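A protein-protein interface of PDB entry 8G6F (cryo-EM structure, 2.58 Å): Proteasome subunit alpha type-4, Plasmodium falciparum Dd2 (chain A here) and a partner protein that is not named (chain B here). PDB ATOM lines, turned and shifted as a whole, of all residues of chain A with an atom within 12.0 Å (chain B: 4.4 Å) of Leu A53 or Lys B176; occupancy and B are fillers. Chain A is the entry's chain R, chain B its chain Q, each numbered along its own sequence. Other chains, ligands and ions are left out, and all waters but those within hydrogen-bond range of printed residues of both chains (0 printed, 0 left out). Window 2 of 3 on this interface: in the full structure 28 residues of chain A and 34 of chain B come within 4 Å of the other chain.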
ATOM      1  N   LYS A  47       2.670 -20.527 -25.926  1.00  0.00           N
ATOM      2  CA  LYS A  47       2.991 -21.432 -24.836  1.00  0.00           C
ATOM      3  C   LYS A  47       3.531 -20.644 -23.651  1.00  0.00           C
ATOM      4  O   LYS A  47       4.178 -19.608 -23.814  1.00  0.00           O
ATOM      5  CB  LYS A  47       4.027 -22.470 -25.269  1.00  0.00           C
ATOM      6  CG  LYS A  47       3.460 -23.640 -26.044  1.00  0.00           C
ATOM      7  CD  LYS A  47       4.565 -24.453 -26.687  1.00  0.00           C
ATOM      8  CE  LYS A  47       5.020 -25.588 -25.793  1.00  0.00           C
ATOM      9  NZ  LYS A  47       6.291 -26.193 -26.270  1.00  0.00           N
ATOM     10  N   LYS A  48       3.258 -21.150 -22.451  1.00  0.00           N
ATOM     11  CA  LYS A  48       3.784 -20.569 -21.216  1.00  0.00           C
ATOM     12  C   LYS A  48       4.230 -21.723 -20.324  1.00  0.00           C
ATOM     13  O   LYS A  48       3.406 -22.357 -19.660  1.00  0.00           O
ATOM     14  CB  LYS A  48       2.744 -19.696 -20.527  1.00  0.00           C
ATOM     15  CG  LYS A  48       2.726 -18.261 -21.030  1.00  0.00           C
ATOM     16  CD  LYS A  48       1.764 -17.393 -20.234  1.00  0.00           C
ATOM     17  CE  LYS A  48       0.319 -17.648 -20.630  1.00  0.00           C
ATOM     18  NZ  LYS A  48       0.018 -17.138 -21.993  1.00  0.00           N
ATOM     19  N   ASN A  49       5.532 -21.994 -20.317  1.00  0.00           N
ATOM     20  CA  ASN A  49       6.106 -23.078 -19.537  1.00  0.00           C
ATOM     21  C   ASN A  49       7.227 -22.538 -18.667  1.00  0.00           C
ATOM     22  O   ASN A  49       7.993 -21.671 -19.096  1.00  0.00           O
ATOM     23  CB  ASN A  49       6.657 -24.187 -20.436  1.00  0.00           C
ATOM     24  CG  ASN A  49       5.568 -25.035 -21.049  1.00  0.00           C
ATOM     25  OD1 ASN A  49       4.954 -25.860 -20.376  1.00  0.00           O
ATOM     26  ND2 ASN A  49       5.321 -24.836 -22.336  1.00  0.00           N
ATOM     27  N   ILE A  50       7.319 -23.053 -17.446  1.00  0.00           N
ATOM     28  CA  ILE A  50       8.466 -22.782 -16.588  1.00  0.00           C
ATOM     29  C   ILE A  50       9.612 -23.650 -17.093  1.00  0.00           C
ATOM     30  O   ILE A  50       9.503 -24.883 -17.068  1.00  0.00           O
ATOM     31  CB  ILE A  50       8.151 -23.070 -15.114  1.00  0.00           C
ATOM     32  CG1 ILE A  50       6.877 -22.338 -14.687  1.00  0.00           C
ATOM     33  CG2 ILE A  50       9.324 -22.668 -14.234  1.00  0.00           C
ATOM     34  CD1 ILE A  50       6.895 -20.854 -14.961  1.00  0.00           C
ATOM     35  N   PRO A  51      10.716 -23.069 -17.561  1.00  0.00           N
ATOM     36  CA  PRO A  51      11.783 -23.895 -18.133  1.00  0.00           C
ATOM     37  C   PRO A  51      12.365 -24.871 -17.121  1.00  0.00           C
ATOM     38  O   PRO A  51      12.499 -24.566 -15.934  1.00  0.00           O
ATOM     39  CB  PRO A  51      12.825 -22.865 -18.582  1.00  0.00           C
ATOM     40  CG  PRO A  51      12.070 -21.607 -18.746  1.00  0.00           C
ATOM     41  CD  PRO A  51      10.999 -21.632 -17.714  1.00  0.00           C
ATOM     42  N   LYS A  52      12.706 -26.060 -17.610  1.00  0.00           N
ATOM     43  CA  LYS A  52      13.474 -27.103 -16.943  1.00  0.00           C
ATOM     44  C   LYS A  52      12.674 -27.849 -15.881  1.00  0.00           C
ATOM     45  O   LYS A  52      13.163 -28.854 -15.371  1.00  0.00           O
ATOM     46  CB  LYS A  52      14.762 -26.565 -16.291  1.00  0.00           C
ATOM     47  CG  LYS A  52      15.730 -27.644 -15.842  1.00  0.00           C
ATOM     48  CD  LYS A  52      17.150 -27.116 -15.769  1.00  0.00           C
ATOM     49  CE  LYS A  52      18.038 -28.036 -14.956  1.00  0.00           C
ATOM     50  NZ  LYS A  52      17.822 -27.854 -13.493  1.00  0.00           N
ATOM     51  N   LEU A  53      11.466 -27.423 -15.543  1.00  0.00           N
ATOM     52  CA  LEU A  53      10.676 -28.088 -14.517  1.00  0.00           C
ATOM     53  C   LEU A  53       9.310 -28.522 -15.011  1.00  0.00           C
ATOM     54  O   LEU A  53       8.838 -29.596 -14.636  1.00  0.00           O
ATOM     55  CB  LEU A  53      10.504 -27.168 -13.301  1.00  0.00           C
ATOM     56  CG  LEU A  53      11.731 -26.886 -12.428  1.00  0.00           C
ATOM     57  CD1 LEU A  53      11.293 -26.344 -11.082  1.00  0.00           C
ATOM     58  CD2 LEU A  53      12.602 -28.114 -12.241  1.00  0.00           C
ATOM     59  N   GLN A  54       8.660 -27.715 -15.838  1.00  0.00           N
ATOM     60  CA  GLN A  54       7.382 -28.094 -16.410  1.00  0.00           C
ATOM     61  C   GLN A  54       7.594 -29.023 -17.595  1.00  0.00           C
ATOM     62  O   GLN A  54       8.624 -28.976 -18.272  1.00  0.00           O
ATOM     63  CB  GLN A  54       6.605 -26.854 -16.849  1.00  0.00           C
ATOM     64  CG  GLN A  54       5.167 -27.129 -17.237  1.00  0.00           C
ATOM     65  CD  GLN A  54       4.248 -25.961 -16.946  1.00  0.00           C
ATOM     66  OE1 GLN A  54       4.687 -24.908 -16.491  1.00  0.00           O
ATOM     67  NE2 GLN A  54       2.964 -26.142 -17.212  1.00  0.00           N
ATOM     68  N   ASN A  55       6.609 -29.883 -17.837  1.00  0.00           N
ATOM     69  CA  ASN A  55       6.646 -30.768 -18.990  1.00  0.00           C
ATOM     70  C   ASN A  55       5.966 -30.063 -20.157  1.00  0.00           C
ATOM     71  O   ASN A  55       4.745 -29.849 -20.107  1.00  0.00           O
ATOM     72  CB  ASN A  55       5.950 -32.082 -18.682  1.00  0.00           C
ATOM     73  CG  ASN A  55       6.299 -33.163 -19.672  1.00  0.00           C
ATOM     74  OD1 ASN A  55       6.800 -32.883 -20.758  1.00  0.00           O
ATOM     75  ND2 ASN A  55       6.037 -34.410 -19.306  1.00  0.00           N
ATOM     76  N   PRO A  56       6.692 -29.685 -21.212  1.00  0.00           N
ATOM     77  CA  PRO A  56       6.053 -28.911 -22.288  1.00  0.00           C
ATOM     78  C   PRO A  56       4.900 -29.629 -22.963  1.00  0.00           C
ATOM     79  O   PRO A  56       3.943 -28.973 -23.392  1.00  0.00           O
ATOM     80  CB  PRO A  56       7.202 -28.656 -23.273  1.00  0.00           C
ATOM     81  CG  PRO A  56       8.445 -28.915 -22.524  1.00  0.00           C
ATOM     82  CD  PRO A  56       8.128 -29.895 -21.456  1.00  0.00           C
ATOM     83  N   LYS A  57       4.955 -30.957 -23.074  1.00  0.00           N
ATOM     84  CA  LYS A  57       3.976 -31.668 -23.887  1.00  0.00           C
ATOM     85  C   LYS A  57       2.600 -31.725 -23.239  1.00  0.00           C
ATOM     86  O   LYS A  57       1.601 -31.861 -23.953  1.00  0.00           O
ATOM     87  CB  LYS A  57       4.482 -33.083 -24.187  1.00  0.00           C
ATOM     88  CG  LYS A  57       4.015 -34.177 -23.227  1.00  0.00           C
ATOM     89  CD  LYS A  57       4.304 -35.559 -23.794  1.00  0.00           C
ATOM     90  CE  LYS A  57       3.135 -36.509 -23.574  1.00  0.00           C
ATOM     91  NZ  LYS A  57       3.281 -37.768 -24.349  1.00  0.00           N
ATOM     92  N   THR A  58       2.516 -31.632 -21.914  1.00  0.00           N
ATOM     93  CA  THR A  58       1.248 -31.889 -21.241  1.00  0.00           C
ATOM     94  C   THR A  58       0.196 -30.866 -21.645  1.00  0.00           C
ATOM     95  O   THR A  58      -0.850 -31.218 -22.201  1.00  0.00           O
ATOM     96  CB  THR A  58       1.450 -31.894 -19.725  1.00  0.00           C
ATOM     97  OG1 THR A  58       2.098 -33.113 -19.337  1.00  0.00           O
ATOM     98  CG2 THR A  58       0.116 -31.781 -19.006  1.00  0.00           C
ATOM     99  N   THR A  59       0.454 -29.592 -21.370  1.00  0.00           N
ATOM    100  CA  THR A  59      -0.493 -28.551 -21.738  1.00  0.00           C
ATOM    101  C   THR A  59      -0.690 -28.538 -23.247  1.00  0.00           C
ATOM    102  O   THR A  59       0.277 -28.578 -24.013  1.00  0.00           O
ATOM    103  CB  THR A  59       0.008 -27.193 -21.255  1.00  0.00           C
ATOM    104  OG1 THR A  59       1.417 -27.091 -21.498  1.00  0.00           O
ATOM    105  CG2 THR A  59      -0.266 -27.024 -19.768  1.00  0.00           C
ATOM    106  N   LYS A 202      10.316 -21.564 -28.216  1.00  0.00           N
ATOM    107  CA  LYS A 202       9.625 -22.310 -27.175  1.00  0.00           C
ATOM    108  C   LYS A 202       8.434 -21.551 -26.607  1.00  0.00           C
ATOM    109  O   LYS A 202       7.833 -22.006 -25.630  1.00  0.00           O
ATOM    110  CB  LYS A 202      10.602 -22.672 -26.052  1.00  0.00           C
ATOM    111  CG  LYS A 202      11.035 -21.496 -25.197  1.00  0.00           C
ATOM    112  CD  LYS A 202      12.545 -21.453 -25.035  1.00  0.00           C
ATOM    113  CE  LYS A 202      13.073 -22.683 -24.316  1.00  0.00           C
ATOM    114  NZ  LYS A 202      14.500 -22.523 -23.927  1.00  0.00           N
ATOM    115  N   TRP B 159       4.677 -31.921 -14.795  1.00  0.00           N
ATOM    116  CA  TRP B 159       5.929 -31.373 -14.304  1.00  0.00           C
ATOM    117  C   TRP B 159       6.983 -32.467 -14.237  1.00  0.00           C
ATOM    118  O   TRP B 159       6.672 -33.656 -14.170  1.00  0.00           O
ATOM    119  CB  TRP B 159       5.757 -30.743 -12.919  1.00  0.00           C
ATOM    120  CG  TRP B 159       4.897 -29.534 -12.930  1.00  0.00           C
ATOM    121  CD1 TRP B 159       3.537 -29.498 -12.936  1.00  0.00           C
ATOM    122  CD2 TRP B 159       5.335 -28.177 -12.945  1.00  0.00           C
ATOM    123  NE1 TRP B 159       3.100 -28.201 -12.952  1.00  0.00           N
ATOM    124  CE2 TRP B 159       4.186 -27.369 -12.958  1.00  0.00           C
ATOM    125  CE3 TRP B 159       6.588 -27.565 -12.949  1.00  0.00           C
ATOM    126  CZ2 TRP B 159       4.253 -25.983 -12.972  1.00  0.00           C
ATOM    127  CZ3 TRP B 159       6.653 -26.194 -12.963  1.00  0.00           C
ATOM    128  CH2 TRP B 159       5.493 -25.416 -12.974  1.00  0.00           C
ATOM    129  N   PHE B 160       8.242 -32.042 -14.275  1.00  0.00           N
ATOM    130  CA  PHE B 160       9.356 -32.921 -13.947  1.00  0.00           C
ATOM    131  C   PHE B 160       9.744 -32.818 -12.482  1.00  0.00           C
ATOM    132  O   PHE B 160      10.217 -33.797 -11.900  1.00  0.00           O
ATOM    133  CB  PHE B 160      10.569 -32.590 -14.818  1.00  0.00           C
ATOM    134  CG  PHE B 160      10.341 -32.796 -16.285  1.00  0.00           C
ATOM    135  CD1 PHE B 160       9.873 -34.002 -16.767  1.00  0.00           C
ATOM    136  CD2 PHE B 160      10.602 -31.782 -17.186  1.00  0.00           C
ATOM    137  CE1 PHE B 160       9.664 -34.190 -18.115  1.00  0.00           C
ATOM    138  CE2 PHE B 160      10.396 -31.967 -18.534  1.00  0.00           C
ATOM    139  CZ  PHE B 160       9.927 -33.171 -18.999  1.00  0.00           C
ATOM    140  N   ALA B 161       9.554 -31.646 -11.880  1.00  0.00           N
ATOM    141  CA  ALA B 161       9.791 -31.444 -10.459  1.00  0.00           C
ATOM    142  C   ALA B 161       9.048 -30.189 -10.042  1.00  0.00           C
ATOM    143  O   ALA B 161       9.126 -29.168 -10.730  1.00  0.00           O
ATOM    144  CB  ALA B 161      11.284 -31.317 -10.156  1.00  0.00           C
ATOM    145  N   SER B 172      10.840 -24.476  -5.258  1.00  0.00           N
ATOM    146  CA  SER B 172      10.943 -24.449  -6.709  1.00  0.00           C
ATOM    147  C   SER B 172      12.305 -23.941  -7.151  1.00  0.00           C
ATOM    148  O   SER B 172      12.878 -24.457  -8.111  1.00  0.00           O
ATOM    149  CB  SER B 172       9.827 -23.591  -7.297  1.00  0.00           C
ATOM    150  OG  SER B 172       8.557 -24.065  -6.893  1.00  0.00           O
ATOM    151  N   SER B 173      12.841 -22.932  -6.467  1.00  0.00           N
ATOM    152  CA  SER B 173      14.178 -22.455  -6.804  1.00  0.00           C
ATOM    153  C   SER B 173      15.221 -23.541  -6.574  1.00  0.00           C
ATOM    154  O   SER B 173      16.106 -23.756  -7.413  1.00  0.00           O
ATOM    155  CB  SER B 173      14.509 -21.208  -5.987  1.00  0.00           C
ATOM    156  OG  SER B 173      14.923 -21.555  -4.679  1.00  0.00           O
ATOM    157  N   VAL B 174      15.126 -24.249  -5.447  1.00  0.00           N
ATOM    158  CA  VAL B 174      16.079 -25.318  -5.161  1.00  0.00           C
ATOM    159  C   VAL B 174      16.003 -26.397  -6.234  1.00  0.00           C
ATOM    160  O   VAL B 174      17.026 -26.863  -6.749  1.00  0.00           O
ATOM    161  CB  VAL B 174      15.821 -25.903  -3.762  1.00  0.00           C
ATOM    162  CG1 VAL B 174      16.655 -27.154  -3.549  1.00  0.00           C
ATOM    163  CG2 VAL B 174      16.116 -24.869  -2.693  1.00  0.00           C
ATOM    164  N   LEU B 175      14.785 -26.815  -6.579  1.00  0.00           N
ATOM    165  CA  LEU B 175      14.619 -27.857  -7.585  1.00  0.00           C
ATOM    166  C   LEU B 175      15.097 -27.386  -8.950  1.00  0.00           C
ATOM    167  O   LEU B 175      15.695 -28.159  -9.701  1.00  0.00           O
ATOM    168  CB  LEU B 175      13.158 -28.295  -7.652  1.00  0.00           C
ATOM    169  CG  LEU B 175      12.695 -29.130  -6.462  1.00  0.00           C
ATOM    170  CD1 LEU B 175      11.188 -29.063  -6.315  1.00  0.00           C
ATOM    171  CD2 LEU B 175      13.162 -30.561  -6.614  1.00  0.00           C
ATOM    172  N   LYS B 176      14.845 -26.126  -9.295  1.00  0.00           N
ATOM    173  CA  LYS B 176      15.331 -25.604 -10.563  1.00  0.00           C
ATOM    174  C   LYS B 176      16.849 -25.645 -10.616  1.00  0.00           C
ATOM    175  O   LYS B 176      17.434 -26.005 -11.644  1.00  0.00           O
ATOM    176  CB  LYS B 176      14.822 -24.177 -10.763  1.00  0.00           C
ATOM    177  CG  LYS B 176      15.339 -23.490 -12.012  1.00  0.00           C
ATOM    178  CD  LYS B 176      14.872 -22.047 -12.078  1.00  0.00           C
ATOM    179  CE  LYS B 176      13.423 -21.941 -12.530  1.00  0.00           C
ATOM    180  NZ  LYS B 176      13.275 -22.109 -14.002  1.00  0.00           N
ATOM    181  N   GLN B 177      17.505 -25.288  -9.513  1.00  0.00           N
ATOM    182  CA  GLN B 177      18.961 -25.231  -9.521  1.00  0.00           C
ATOM    183  C   GLN B 177      19.602 -26.612  -9.455  1.00  0.00           C
ATOM    184  O   GLN B 177      20.715 -26.790  -9.960  1.00  0.00           O
ATOM    185  CB  GLN B 177      19.451 -24.359  -8.361  1.00  0.00           C
ATOM    186  CG  GLN B 177      19.826 -25.120  -7.100  1.00  0.00           C
ATOM    187  CD  GLN B 177      19.769 -24.252  -5.858  1.00  0.00           C
ATOM    188  OE1 GLN B 177      19.738 -23.026  -5.945  1.00  0.00           O
ATOM    189  NE2 GLN B 177      19.749 -24.887  -4.691  1.00  0.00           N
ATOM    190  N   GLU B 178      18.931 -27.598  -8.857  1.00  0.00           N
ATOM    191  CA  GLU B 178      19.566 -28.884  -8.580  1.00  0.00           C
ATOM    192  C   GLU B 178      19.069 -30.041  -9.435  1.00  0.00           C
ATOM    193  O   GLU B 178      19.857 -30.936  -9.742  1.00  0.00           O
ATOM    194  CB  GLU B 178      19.371 -29.252  -7.104  1.00  0.00           C
ATOM    195  CG  GLU B 178      20.350 -28.572  -6.167  1.00  0.00           C
ATOM    196  CD  GLU B 178      21.278 -29.555  -5.479  1.00  0.00           C
ATOM    197  OE1 GLU B 178      21.847 -30.426  -6.171  1.00  0.00           O
ATOM    198  OE2 GLU B 178      21.443 -29.455  -4.244  1.00  0.00           O
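N of Phe B160 lies within hydrogen-bond range of O of Leu A53. The backbone carbonyl oxygen (O) of Pro A51 sits at hydrogen-bond distance from the side-chain amino group (NZ) of Lys B176 (3.2 Å). The backbone carbonyl oxygen of Lys B176 is in hydrogen-bond range of the side-chain amino group of Lys A52.
The side-chain amide oxygen of Gln A54 is in hydrogen-bond range of the backbone NH of Ile A50 (3.4 Å).
Ile A50 touches Trp B159 (CG1 to CH2, 3.8 Å). Lys B176 touches Ile A50 (NZ to CG2, 3.997 Å). O of Leu A53 touches CA of Trp B159, 3.4 Å away. O of Leu A53 touches N of Ala B161, at 3.5 Å. O of Ser B172 touches CD1 of Leu A53 (3.9 Å). CD1 of Leu A53 touches N of Lys B176 (3.98 Å). CE3 of Trp B159 touches N of Gln A54, 3.6 Å away. O of Gln A54 touches CE2 of Phe B160, 3.5 Å away. Asn A55 touches Trp B159. CZ of Phe B160 touches OD1 of Asn A55, at 3.6 Å.
Of the printed residues of chain B, Leu A53 touches Trp B159, Phe B160, Ala B161, Ser B172 and Lys B176. Printed residues of chain A within 4 Å of Lys B176: Ile A50, Pro A51, Lys A52 and Leu A53. Trp B159 touches four residues of chain A. Phe B160 touches just these residues of chain A: Leu A53, Gln A54 and Asn A55. Of chain A, only Leu A53 (3.9 Å) comes within 4 Å of Ser B172. No residue of chain A comes within 4 Å of Ser B173. No residue of chain A comes within 4 Å of Val B174. Gln B177 touches none of the printed residues of chain A. Of the printed residues of chain B, Asn A55 touches Trp B159 and Phe B160. Printed residues of chain B within 4 Å of Gln A54: Trp B159 (3.6 Å) and Phe B160 (3.5 Å). Printed residues of chain B within 4 Å of Ile A50: Trp B159 and Lys B176. Of the printed residues of chain B, Lys A52 touches Lys B176. Of the printed residues of chain B, Pro A51 touches Lys B176. Thr A59 touches none of the printed residues of chain B. The nearest printed residue of chain B that does not touch Leu A53 is Leu B175 (4.003 Å). The nearest printed residue of chain A that does not touch Lys B176 is Asn A49 (7.4 Å).
Of the 10 printed residues of chain B, 5 touch a printed residue of chain A. Printed residues of chain B that touch a printed residue of chain A: Trp B159, Phe B160, Ala B161, Ser B172 and Lys B176. Along chain A the printed residues that touch a printed residue of chain B span positions 50 to 55. Among the printed residues, no Asp or Glu carboxylate lies within 4 Å of a Lys or Arg side-chain nitrogen of the other chain.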
